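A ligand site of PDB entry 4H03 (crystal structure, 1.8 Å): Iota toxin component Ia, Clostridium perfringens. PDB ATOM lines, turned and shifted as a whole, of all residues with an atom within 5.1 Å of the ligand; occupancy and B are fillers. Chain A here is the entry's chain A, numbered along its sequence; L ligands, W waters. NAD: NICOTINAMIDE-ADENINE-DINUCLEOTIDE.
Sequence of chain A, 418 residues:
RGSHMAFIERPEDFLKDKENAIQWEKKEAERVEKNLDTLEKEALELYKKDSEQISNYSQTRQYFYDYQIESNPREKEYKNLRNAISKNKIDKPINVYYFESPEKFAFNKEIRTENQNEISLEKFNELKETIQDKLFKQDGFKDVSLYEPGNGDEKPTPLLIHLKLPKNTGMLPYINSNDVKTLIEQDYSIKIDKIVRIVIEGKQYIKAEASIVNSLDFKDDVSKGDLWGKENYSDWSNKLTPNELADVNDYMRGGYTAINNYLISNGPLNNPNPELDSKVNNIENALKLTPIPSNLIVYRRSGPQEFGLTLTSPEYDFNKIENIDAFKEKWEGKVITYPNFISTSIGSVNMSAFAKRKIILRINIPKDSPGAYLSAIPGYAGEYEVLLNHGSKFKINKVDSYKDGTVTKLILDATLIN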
ATOM      1  N   TYR A 256     -31.214  12.847 -10.014  1.00  0.00           N
ATOM      2  CA  TYR A 256     -29.782  12.994 -10.303  1.00  0.00           C
ATOM      3  C   TYR A 256     -28.865  12.485  -9.187  1.00  0.00           C
ATOM      4  O   TYR A 256     -27.806  11.937  -9.483  1.00  0.00           O
ATOM      5  CB  TYR A 256     -29.420  14.439 -10.707  1.00  0.00           C
ATOM      6  CG  TYR A 256     -29.528  15.548  -9.677  1.00  0.00           C
ATOM      7  CD1 TYR A 256     -30.610  16.425  -9.674  1.00  0.00           C
ATOM      8  CD2 TYR A 256     -28.507  15.770  -8.755  1.00  0.00           C
ATOM      9  CE1 TYR A 256     -30.689  17.464  -8.755  1.00  0.00           C
ATOM     10  CE2 TYR A 256     -28.586  16.809  -7.836  1.00  0.00           C
ATOM     11  CZ  TYR A 256     -29.681  17.651  -7.836  1.00  0.00           C
ATOM     12  OH  TYR A 256     -29.765  18.675  -6.925  1.00  0.00           O
ATOM     13  N   ASN A 260     -26.298   9.746 -10.212  1.00  0.00           N
ATOM     14  CA  ASN A 260     -24.903  10.136 -10.244  1.00  0.00           C
ATOM     15  C   ASN A 260     -24.055   9.404  -9.204  1.00  0.00           C
ATOM     16  O   ASN A 260     -22.887   9.115  -9.457  1.00  0.00           O
ATOM     17  CB  ASN A 260     -24.747  11.658 -10.109  1.00  0.00           C
ATOM     18  CG  ASN A 260     -25.191  12.423 -11.360  1.00  0.00           C
ATOM     19  OD1 ASN A 260     -25.281  11.858 -12.444  1.00  0.00           O
ATOM     20  ND2 ASN A 260     -25.469  13.708 -11.195  1.00  0.00           N
ATOM     21  N   ILE A 264     -20.717   7.403  -9.925  1.00  0.00           N
ATOM     22  CA  ILE A 264     -19.458   7.706  -9.223  1.00  0.00           C
ATOM     23  C   ILE A 264     -18.927   6.494  -8.442  1.00  0.00           C
ATOM     24  O   ILE A 264     -17.711   6.271  -8.397  1.00  0.00           O
ATOM     25  CB  ILE A 264     -19.613   8.939  -8.304  1.00  0.00           C
ATOM     26  CG1 ILE A 264     -19.811  10.191  -9.167  1.00  0.00           C
ATOM     27  CG2 ILE A 264     -18.380   9.144  -7.424  1.00  0.00           C
ATOM     28  CD1 ILE A 264     -20.373  11.380  -8.405  1.00  0.00           C
ATOM     29  N   TYR A 299     -20.423  27.740 -17.263  1.00  0.00           N
ATOM     30  CA  TYR A 299     -19.868  28.029 -15.952  1.00  0.00           C
ATOM     31  C   TYR A 299     -20.461  27.073 -14.938  1.00  0.00           C
ATOM     32  O   TYR A 299     -21.658  26.759 -14.983  1.00  0.00           O
ATOM     33  CB  TYR A 299     -20.178  29.479 -15.567  1.00  0.00           C
ATOM     34  CG  TYR A 299     -19.569  30.493 -16.519  1.00  0.00           C
ATOM     35  CD1 TYR A 299     -20.171  30.781 -17.743  1.00  0.00           C
ATOM     36  CD2 TYR A 299     -18.373  31.141 -16.193  1.00  0.00           C
ATOM     37  CE1 TYR A 299     -19.601  31.704 -18.610  1.00  0.00           C
ATOM     38  CE2 TYR A 299     -17.801  32.054 -17.056  1.00  0.00           C
ATOM     39  CZ  TYR A 299     -18.414  32.334 -18.269  1.00  0.00           C
ATOM     40  OH  TYR A 299     -17.836  33.252 -19.121  1.00  0.00           O
ATOM     41  N   ARG A 300     -19.633  26.584 -14.018  1.00  0.00           N
ATOM     42  CA  ARG A 300     -20.103  25.744 -12.920  1.00  0.00           C
ATOM     43  C   ARG A 300     -19.458  26.210 -11.631  1.00  0.00           C
ATOM     44  O   ARG A 300     -18.239  26.377 -11.585  1.00  0.00           O
ATOM     45  CB  ARG A 300     -19.762  24.270 -13.179  1.00  0.00           C
ATOM     46  CG  ARG A 300     -19.804  23.388 -11.931  1.00  0.00           C
ATOM     47  CD  ARG A 300     -19.674  21.907 -12.270  1.00  0.00           C
ATOM     48  NE  ARG A 300     -19.844  21.111 -11.056  1.00  0.00           N
ATOM     49  CZ  ARG A 300     -21.012  20.766 -10.513  1.00  0.00           C
ATOM     50  NH1 ARG A 300     -22.161  21.099 -11.090  1.00  0.00           N
ATOM     51  NH2 ARG A 300     -21.035  20.054  -9.394  1.00  0.00           N
ATOM     52  N   ARG A 301     -20.253  26.429 -10.600  1.00  0.00           N
ATOM     53  CA  ARG A 301     -19.678  26.672  -9.278  1.00  0.00           C
ATOM     54  C   ARG A 301     -19.559  25.323  -8.582  1.00  0.00           C
ATOM     55  O   ARG A 301     -20.553  24.735  -8.148  1.00  0.00           O
ATOM     56  CB  ARG A 301     -20.482  27.689  -8.475  1.00  0.00           C
ATOM     57  CG  ARG A 301     -20.686  28.982  -9.254  1.00  0.00           C
ATOM     58  CD  ARG A 301     -20.454  30.231  -8.447  1.00  0.00           C
ATOM     59  NE  ARG A 301     -20.438  31.375  -9.364  1.00  0.00           N
ATOM     60  CZ  ARG A 301     -19.957  32.580  -9.082  1.00  0.00           C
ATOM     61  NH1 ARG A 301     -19.449  32.869  -7.894  1.00  0.00           N
ATOM     62  NH2 ARG A 301     -19.992  33.505 -10.017  1.00  0.00           N
ATOM     63  N   SER A 302     -18.321  24.844  -8.510  1.00  0.00           N
ATOM     64  CA  SER A 302     -18.026  23.523  -7.980  1.00  0.00           C
ATOM     65  C   SER A 302     -18.040  23.502  -6.466  1.00  0.00           C
ATOM     66  O   SER A 302     -17.614  24.462  -5.812  1.00  0.00           O
ATOM     67  CB  SER A 302     -16.650  23.039  -8.457  1.00  0.00           C
ATOM     68  OG  SER A 302     -16.686  22.687  -9.826  1.00  0.00           O
ATOM     69  N   GLY A 303     -18.498  22.389  -5.918  1.00  0.00           N
ATOM     70  CA  GLY A 303     -18.295  22.112  -4.508  1.00  0.00           C
ATOM     71  C   GLY A 303     -16.840  21.712  -4.312  1.00  0.00           C
ATOM     72  O   GLY A 303     -16.209  21.202  -5.248  1.00  0.00           O
ATOM     73  N   PRO A 304     -16.300  21.929  -3.100  1.00  0.00           N
ATOM     74  CA  PRO A 304     -14.898  21.575  -2.902  1.00  0.00           C
ATOM     75  C   PRO A 304     -14.618  20.075  -3.039  1.00  0.00           C
ATOM     76  O   PRO A 304     -13.472  19.697  -3.290  1.00  0.00           O
ATOM     77  CB  PRO A 304     -14.613  22.064  -1.474  1.00  0.00           C
ATOM     78  CG  PRO A 304     -15.951  22.168  -0.814  1.00  0.00           C
ATOM     79  CD  PRO A 304     -16.879  22.581  -1.923  1.00  0.00           C
ATOM     80  N   GLN A 305     -15.641  19.234  -2.889  1.00  0.00           N
ATOM     81  CA  GLN A 305     -15.451  17.794  -2.918  1.00  0.00           C
ATOM     82  C   GLN A 305     -14.969  17.299  -4.296  1.00  0.00           C
ATOM     83  O   GLN A 305     -14.267  16.289  -4.387  1.00  0.00           O
ATOM     84  CB  GLN A 305     -16.716  17.059  -2.480  1.00  0.00           C
ATOM     85  CG  GLN A 305     -17.098  17.311  -1.012  1.00  0.00           C
ATOM     86  CD  GLN A 305     -17.891  18.595  -0.788  1.00  0.00           C
ATOM     87  OE1 GLN A 305     -18.160  19.355  -1.724  1.00  0.00           O
ATOM     88  NE2 GLN A 305     -18.258  18.844   0.466  1.00  0.00           N
ATOM     89  N   GLU A 306     -15.351  18.019  -5.350  1.00  0.00           N
ATOM     90  CA  GLU A 306     -14.857  17.734  -6.720  1.00  0.00           C
ATOM     91  C   GLU A 306     -13.356  17.903  -6.865  1.00  0.00           C
ATOM     92  O   GLU A 306     -12.768  17.436  -7.840  1.00  0.00           O
ATOM     93  CB  GLU A 306     -15.525  18.656  -7.727  1.00  0.00           C
ATOM     94  CG  GLU A 306     -16.986  18.356  -7.974  1.00  0.00           C
ATOM     95  CD  GLU A 306     -17.729  19.547  -8.525  1.00  0.00           C
ATOM     96  OE1 GLU A 306     -17.355  20.030  -9.619  1.00  0.00           O
ATOM     97  OE2 GLU A 306     -18.689  20.011  -7.866  1.00  0.00           O
ATOM     98  N   THR A 337     -11.921  13.944 -14.780  1.00  0.00           N
ATOM     99  CA  THR A 337     -13.060  13.223 -15.349  1.00  0.00           C
ATOM    100  C   THR A 337     -14.171  13.084 -14.312  1.00  0.00           C
ATOM    101  O   THR A 337     -13.922  12.824 -13.134  1.00  0.00           O
ATOM    102  CB  THR A 337     -12.651  11.860 -15.943  1.00  0.00           C
ATOM    103  OG1 THR A 337     -13.767  11.275 -16.618  1.00  0.00           O
ATOM    104  CG2 THR A 337     -12.168  10.919 -14.884  1.00  0.00           C
ATOM    105  N   TYR A 338     -15.399  13.304 -14.787  1.00  0.00           N
ATOM    106  CA  TYR A 338     -16.606  13.196 -13.974  1.00  0.00           C
ATOM    107  C   TYR A 338     -17.390  11.974 -14.436  1.00  0.00           C
ATOM    108  O   TYR A 338     -17.916  11.970 -15.551  1.00  0.00           O
ATOM    109  CB  TYR A 338     -17.485  14.446 -14.147  1.00  0.00           C
ATOM    110  CG  TYR A 338     -17.006  15.685 -13.406  1.00  0.00           C
ATOM    111  CD1 TYR A 338     -17.676  16.143 -12.278  1.00  0.00           C
ATOM    112  CD2 TYR A 338     -15.890  16.387 -13.844  1.00  0.00           C
ATOM    113  CE1 TYR A 338     -17.241  17.265 -11.599  1.00  0.00           C
ATOM    114  CE2 TYR A 338     -15.453  17.515 -13.177  1.00  0.00           C
ATOM    115  CZ  TYR A 338     -16.129  17.959 -12.056  1.00  0.00           C
ATOM    116  OH  TYR A 338     -15.691  19.078 -11.386  1.00  0.00           O
ATOM    117  N   PRO A 339     -17.478  10.934 -13.587  1.00  0.00           N
ATOM    118  CA  PRO A 339     -18.319   9.782 -13.958  1.00  0.00           C
ATOM    119  C   PRO A 339     -19.791  10.147 -13.983  1.00  0.00           C
ATOM    120  O   PRO A 339     -20.572   9.527 -14.712  1.00  0.00           O
ATOM    121  CB  PRO A 339     -18.031   8.742 -12.856  1.00  0.00           C
ATOM    122  CG  PRO A 339     -16.932   9.298 -12.024  1.00  0.00           C
ATOM    123  CD  PRO A 339     -16.853  10.772 -12.267  1.00  0.00           C
ATOM    124  N   ASN A 340     -20.159  11.149 -13.190  1.00  0.00           N
ATOM    125  CA  ASN A 340     -21.521  11.677 -13.173  1.00  0.00           C
ATOM    126  C   ASN A 340     -21.832  12.612 -14.344  1.00  0.00           C
ATOM    127  O   ASN A 340     -20.924  13.180 -14.938  1.00  0.00           O
ATOM    128  CB  ASN A 340     -21.799  12.432 -11.844  1.00  0.00           C
ATOM    129  CG  ASN A 340     -20.692  13.413 -11.459  1.00  0.00           C
ATOM    130  OD1 ASN A 340     -19.497  13.144 -11.612  1.00  0.00           O
ATOM    131  ND2 ASN A 340     -21.093  14.555 -10.909  1.00  0.00           N
ATOM    132  N   SER A 343     -23.909  19.381 -14.161  1.00  0.00           N
ATOM    133  CA  SER A 343     -24.644  20.614 -14.406  1.00  0.00           C
ATOM    134  C   SER A 343     -23.716  21.820 -14.553  1.00  0.00           C
ATOM    135  O   SER A 343     -22.782  22.006 -13.776  1.00  0.00           O
ATOM    136  CB  SER A 343     -25.630  20.896 -13.278  1.00  0.00           C
ATOM    137  OG  SER A 343     -26.635  19.905 -13.247  1.00  0.00           O
ATOM    138  N   THR A 344     -24.019  22.621 -15.568  1.00  0.00           N
ATOM    139  CA  THR A 344     -23.355  23.887 -15.822  1.00  0.00           C
ATOM    140  C   THR A 344     -24.407  24.917 -16.223  1.00  0.00           C
ATOM    141  O   THR A 344     -25.559  24.576 -16.498  1.00  0.00           O
ATOM    142  CB  THR A 344     -22.331  23.778 -16.966  1.00  0.00           C
ATOM    143  OG1 THR A 344     -23.022  23.559 -18.209  1.00  0.00           O
ATOM    144  CG2 THR A 344     -21.376  22.632 -16.719  1.00  0.00           C
ATOM    145  N   SER A 345     -23.986  26.175 -16.262  1.00  0.00           N
ATOM    146  CA  SER A 345     -24.864  27.277 -16.625  1.00  0.00           C
ATOM    147  C   SER A 345     -24.301  28.088 -17.785  1.00  0.00           C
ATOM    148  O   SER A 345     -23.085  28.211 -17.965  1.00  0.00           O
ATOM    149  CB  SER A 345     -25.061  28.209 -15.431  1.00  0.00           C
ATOM    150  OG  SER A 345     -25.939  29.281 -15.762  1.00  0.00           O
ATOM    151  N   PHE A 354     -25.420  28.975  -4.543  1.00  0.00           N
ATOM    152  CA  PHE A 354     -23.988  28.698  -4.471  1.00  0.00           C
ATOM    153  C   PHE A 354     -23.126  29.944  -4.257  1.00  0.00           C
ATOM    154  O   PHE A 354     -21.984  30.022  -4.728  1.00  0.00           O
ATOM    155  CB  PHE A 354     -23.543  27.891  -5.690  1.00  0.00           C
ATOM    156  CG  PHE A 354     -23.929  28.474  -7.016  1.00  0.00           C
ATOM    157  CD1 PHE A 354     -24.572  27.683  -7.965  1.00  0.00           C
ATOM    158  CD2 PHE A 354     -23.623  29.784  -7.357  1.00  0.00           C
ATOM    159  CE1 PHE A 354     -24.908  28.191  -9.197  1.00  0.00           C
ATOM    160  CE2 PHE A 354     -23.960  30.301  -8.592  1.00  0.00           C
ATOM    161  CZ  PHE A 354     -24.606  29.498  -9.516  1.00  0.00           C
ATOM    162  N   ARG A 357     -19.530  29.273  -2.800  1.00  0.00           N
ATOM    163  CA  ARG A 357     -18.628  28.326  -3.456  1.00  0.00           C
ATOM    164  C   ARG A 357     -17.446  29.075  -4.054  1.00  0.00           C
ATOM    165  O   ARG A 357     -17.624  30.136  -4.660  1.00  0.00           O
ATOM    166  CB  ARG A 357     -19.360  27.539  -4.531  1.00  0.00           C
ATOM    167  CG  ARG A 357     -20.237  26.448  -3.959  1.00  0.00           C
ATOM    168  CD  ARG A 357     -20.793  25.528  -5.026  1.00  0.00           C
ATOM    169  NE  ARG A 357     -21.387  24.347  -4.407  1.00  0.00           N
ATOM    170  CZ  ARG A 357     -21.983  23.359  -5.069  1.00  0.00           C
ATOM    171  NH1 ARG A 357     -22.070  23.363  -6.387  1.00  0.00           N
ATOM    172  NH2 ARG A 357     -22.499  22.330  -4.391  1.00  0.00           N
ATOM    173  N   GLU A 383     -32.232  28.067 -13.789  1.00  0.00           N
ATOM    174  CA  GLU A 383     -30.860  27.521 -13.689  1.00  0.00           C
ATOM    175  C   GLU A 383     -29.978  27.999 -14.852  1.00  0.00           C
ATOM    176  O   GLU A 383     -28.748  28.055 -14.732  1.00  0.00           O
ATOM    177  CB  GLU A 383     -30.853  25.980 -13.682  1.00  0.00           C
ATOM    178  CG  GLU A 383     -32.136  25.262 -13.277  1.00  0.00           C
ATOM    179  CD  GLU A 383     -32.398  25.241 -11.781  1.00  0.00           C
ATOM    180  OE1 GLU A 383     -33.587  25.178 -11.394  1.00  0.00           O
ATOM    181  OE2 GLU A 383     -31.434  25.285 -10.991  1.00  0.00           O
ATOM    182  N   GLU A 385     -29.528  26.165 -17.441  1.00  0.00           N
ATOM    183  CA  GLU A 385     -28.701  24.977 -17.338  1.00  0.00           C
ATOM    184  C   GLU A 385     -28.367  24.306 -18.668  1.00  0.00           C
ATOM    185  O   GLU A 385     -29.250  24.092 -19.509  1.00  0.00           O
ATOM    186  CB  GLU A 385     -29.373  23.930 -16.447  1.00  0.00           C
ATOM    187  CG  GLU A 385     -28.533  22.684 -16.189  1.00  0.00           C
ATOM    188  CD  GLU A 385     -29.219  21.704 -15.260  1.00  0.00           C
ATOM    189  OE1 GLU A 385     -28.533  20.772 -14.769  1.00  0.00           O
ATOM    190  OE2 GLU A 385     -30.429  21.857 -15.006  1.00  0.00           O
HETATM  191  PA  NAD L   1     -23.908  18.095  -7.764  1.00  0.00           P
HETATM  192  O1A NAD L   1     -24.940  16.985  -7.723  1.00  0.00           O
HETATM  193  O2A NAD L   1     -23.075  18.361  -9.012  1.00  0.00           O
HETATM  194  O5B NAD L   1     -22.912  17.967  -6.501  1.00  0.00           O
HETATM  195  C5B NAD L   1     -23.347  17.462  -5.243  1.00  0.00           C
HETATM  196  C4B NAD L   1     -22.103  17.243  -4.402  1.00  0.00           C
HETATM  197  O4B NAD L   1     -21.281  16.239  -5.008  1.00  0.00           O
HETATM  198  C3B NAD L   1     -21.234  18.495  -4.320  1.00  0.00           C
HETATM  199  O3B NAD L   1     -20.595  18.545  -3.045  1.00  0.00           O
HETATM  200  C2B NAD L   1     -20.201  18.306  -5.422  1.00  0.00           C
HETATM  201  O2B NAD L   1     -18.983  19.001  -5.149  1.00  0.00           O
HETATM  202  C1B NAD L   1     -20.008  16.815  -5.357  1.00  0.00           C
HETATM  203  N9A NAD L   1     -19.558  16.141  -6.597  1.00  0.00           N
HETATM  204  C8A NAD L   1     -20.187  16.155  -7.791  1.00  0.00           C
HETATM  205  N7A NAD L   1     -19.498  15.400  -8.683  1.00  0.00           N
HETATM  206  C5A NAD L   1     -18.427  14.894  -8.049  1.00  0.00           C
HETATM  207  C6A NAD L   1     -17.297  14.014  -8.420  1.00  0.00           C
HETATM  208  N6A NAD L   1     -17.223  13.545  -9.685  1.00  0.00           N
HETATM  209  N1A NAD L   1     -16.384  13.714  -7.463  1.00  0.00           N
HETATM  210  C2A NAD L   1     -16.481  14.192  -6.196  1.00  0.00           C
HETATM  211  N3A NAD L   1     -17.495  15.001  -5.800  1.00  0.00           N
HETATM  212  C4A NAD L   1     -18.465  15.370  -6.666  1.00  0.00           C
HETATM  213  O3  NAD L   1     -24.685  19.412  -7.262  1.00  0.00           O
HETATM  214  PN  NAD L   1     -24.682  20.845  -7.984  1.00  0.00           P
HETATM  215  O1N NAD L   1     -24.144  20.760  -9.385  1.00  0.00           O
HETATM  216  O2N NAD L   1     -24.087  21.898  -6.950  1.00  0.00           O
HETATM  217  O5D NAD L   1     -26.257  21.085  -7.986  1.00  0.00           O
HETATM  218  C5D NAD L   1     -27.062  20.581  -9.024  1.00  0.00           C
HETATM  219  C4D NAD L   1     -28.312  21.405  -8.866  1.00  0.00           C
HETATM  220  O4D NAD L   1     -28.016  22.789  -9.092  1.00  0.00           O
HETATM  221  C3D NAD L   1     -29.263  20.975  -9.938  1.00  0.00           C
HETATM  222  O3D NAD L   1     -30.610  21.270  -9.543  1.00  0.00           O
HETATM  223  C2D NAD L   1     -28.827  21.841 -11.099  1.00  0.00           C
HETATM  224  O2D NAD L   1     -29.895  22.063 -12.031  1.00  0.00           O
HETATM  225  C1D NAD L   1     -28.355  23.136 -10.435  1.00  0.00           C
HETATM  226  N1N NAD L   1     -27.242  23.795 -11.154  1.00  0.00           N
HETATM  227  C2N NAD L   1     -26.027  23.962 -10.594  1.00  0.00           C
HETATM  228  C3N NAD L   1     -24.982  24.585 -11.299  1.00  0.00           C
HETATM  229  C7N NAD L   1     -23.621  24.802 -10.692  1.00  0.00           C
HETATM  230  O7N NAD L   1     -22.912  25.701 -11.106  1.00  0.00           O
HETATM  231  N7N NAD L   1     -23.187  24.030  -9.682  1.00  0.00           N
HETATM  232  C4N NAD L   1     -25.236  25.053 -12.581  1.00  0.00           C
HETATM  233  C5N NAD L   1     -26.502  24.879 -13.142  1.00  0.00           C
HETATM  234  C6N NAD L   1     -27.490  24.248 -12.396  1.00  0.00           C
HETATM  235  O   HOH W   1     -21.412  17.486 -11.200  1.00  0.00           O
HETATM  236  O   HOH W   2     -26.434  15.228  -5.705  1.00  0.00           O
HETATM  237  O   HOH W   3     -14.878  11.154  -7.488  1.00  0.00           O
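NH1 of Arg 357 lies within salt-bridge range of O2N of the ligand, 2.6 Å away.
The guanidinium group (NH1) of Arg 300 lies within salt-bridge range of an oxygen (O1N) of the ligand (2.6 Å).
O7N of the ligand lies within hydrogen-bond range of N of Arg 301 (2.8 Å).
The backbone carbonyl oxygen of Arg 301 is in hydrogen-bond range of a nitrogen (N7N) of the ligand (3.1 Å).
ND2 of Asn 340 lies within hydrogen-bond range of N7A of the ligand (2.9 Å).
An oxygen (O3B) of the ligand sits at hydrogen-bond distance from the side-chain amide oxygen of Gln 305.
OE2 of Glu 306 is in hydrogen-bond range of O2B of the ligand (2.9 Å).
O2D of the ligand sits at hydrogen-bond distance from OE2 of Glu 385 (3.0 Å).
The backbone carbonyl oxygen (O) of Arg 301 lies within hydrogen-bond range of the guanidinium group (NH1) of Arg 357.
The guanidinium group of Arg 300 lies within hydrogen-bond range of the backbone carbonyl oxygen of Ser 343.
The side-chain carboxylate (OE2) of Glu 306 sits at hydrogen-bond distance from the backbone NH (N) of Gly 303.
OE1 of Glu 306 is in hydrogen-bond range of OH of Tyr 338 (2.6 Å).
OE1 of Glu 306 is in hydrogen-bond range of OG of Ser 302.
OE1 of Glu 385 sits at hydrogen-bond distance from OG of Ser 343, at 2.6 Å.
O of Tyr 256 sits close to ND2 of Asn 260.
The backbone carbonyl oxygen (O) of Glu 383 sits at hydrogen-bond distance from the side-chain hydroxyl (OG) of Ser 345, at 3.2 Å.
Tyr 256 touches the ligand (OH to C4D, 3.7 Å).
CA of Gly 303 touches O2B of the ligand, at 3.3 Å.
Tyr 338 touches the ligand (CD1 to N6A, 3.7 Å).
CD of Pro 339 touches N6A of the ligand (3.8 Å).
Ser 343 touches the ligand (OG to C2D, 3.6 Å).
O of Thr 344 touches C5N of the ligand, at 3.5 Å.
Phe 354 touches the ligand (CE1 to O7N, 3.7 Å).
Glu 383 touches the ligand.
Hydrophobic or aromatic side chains within 4 Å of the ligand: Tyr 256, Tyr 338, Pro 339 and Phe 354.
15 residues have an atom within 4 Å of the ligand: Tyr 256, Arg 300, Arg 301, Gly 303, Gln 305, Glu 306, Tyr 338, Pro 339, Asn 340, Ser 343, Thr 344, Phe 354, Arg 357, Glu 383 and Glu 385.
The nearest printed residue that does not touch the ligand is Ile 264 (4.03 Å).
Water W1 lies within hydrogen-bond range of an oxygen (O2A) of the ligand (2.9 Å), the side-chain amide nitrogen of Asn 340 (3.0 Å) and the guanidinium group of Arg 300 (3.2 Å).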
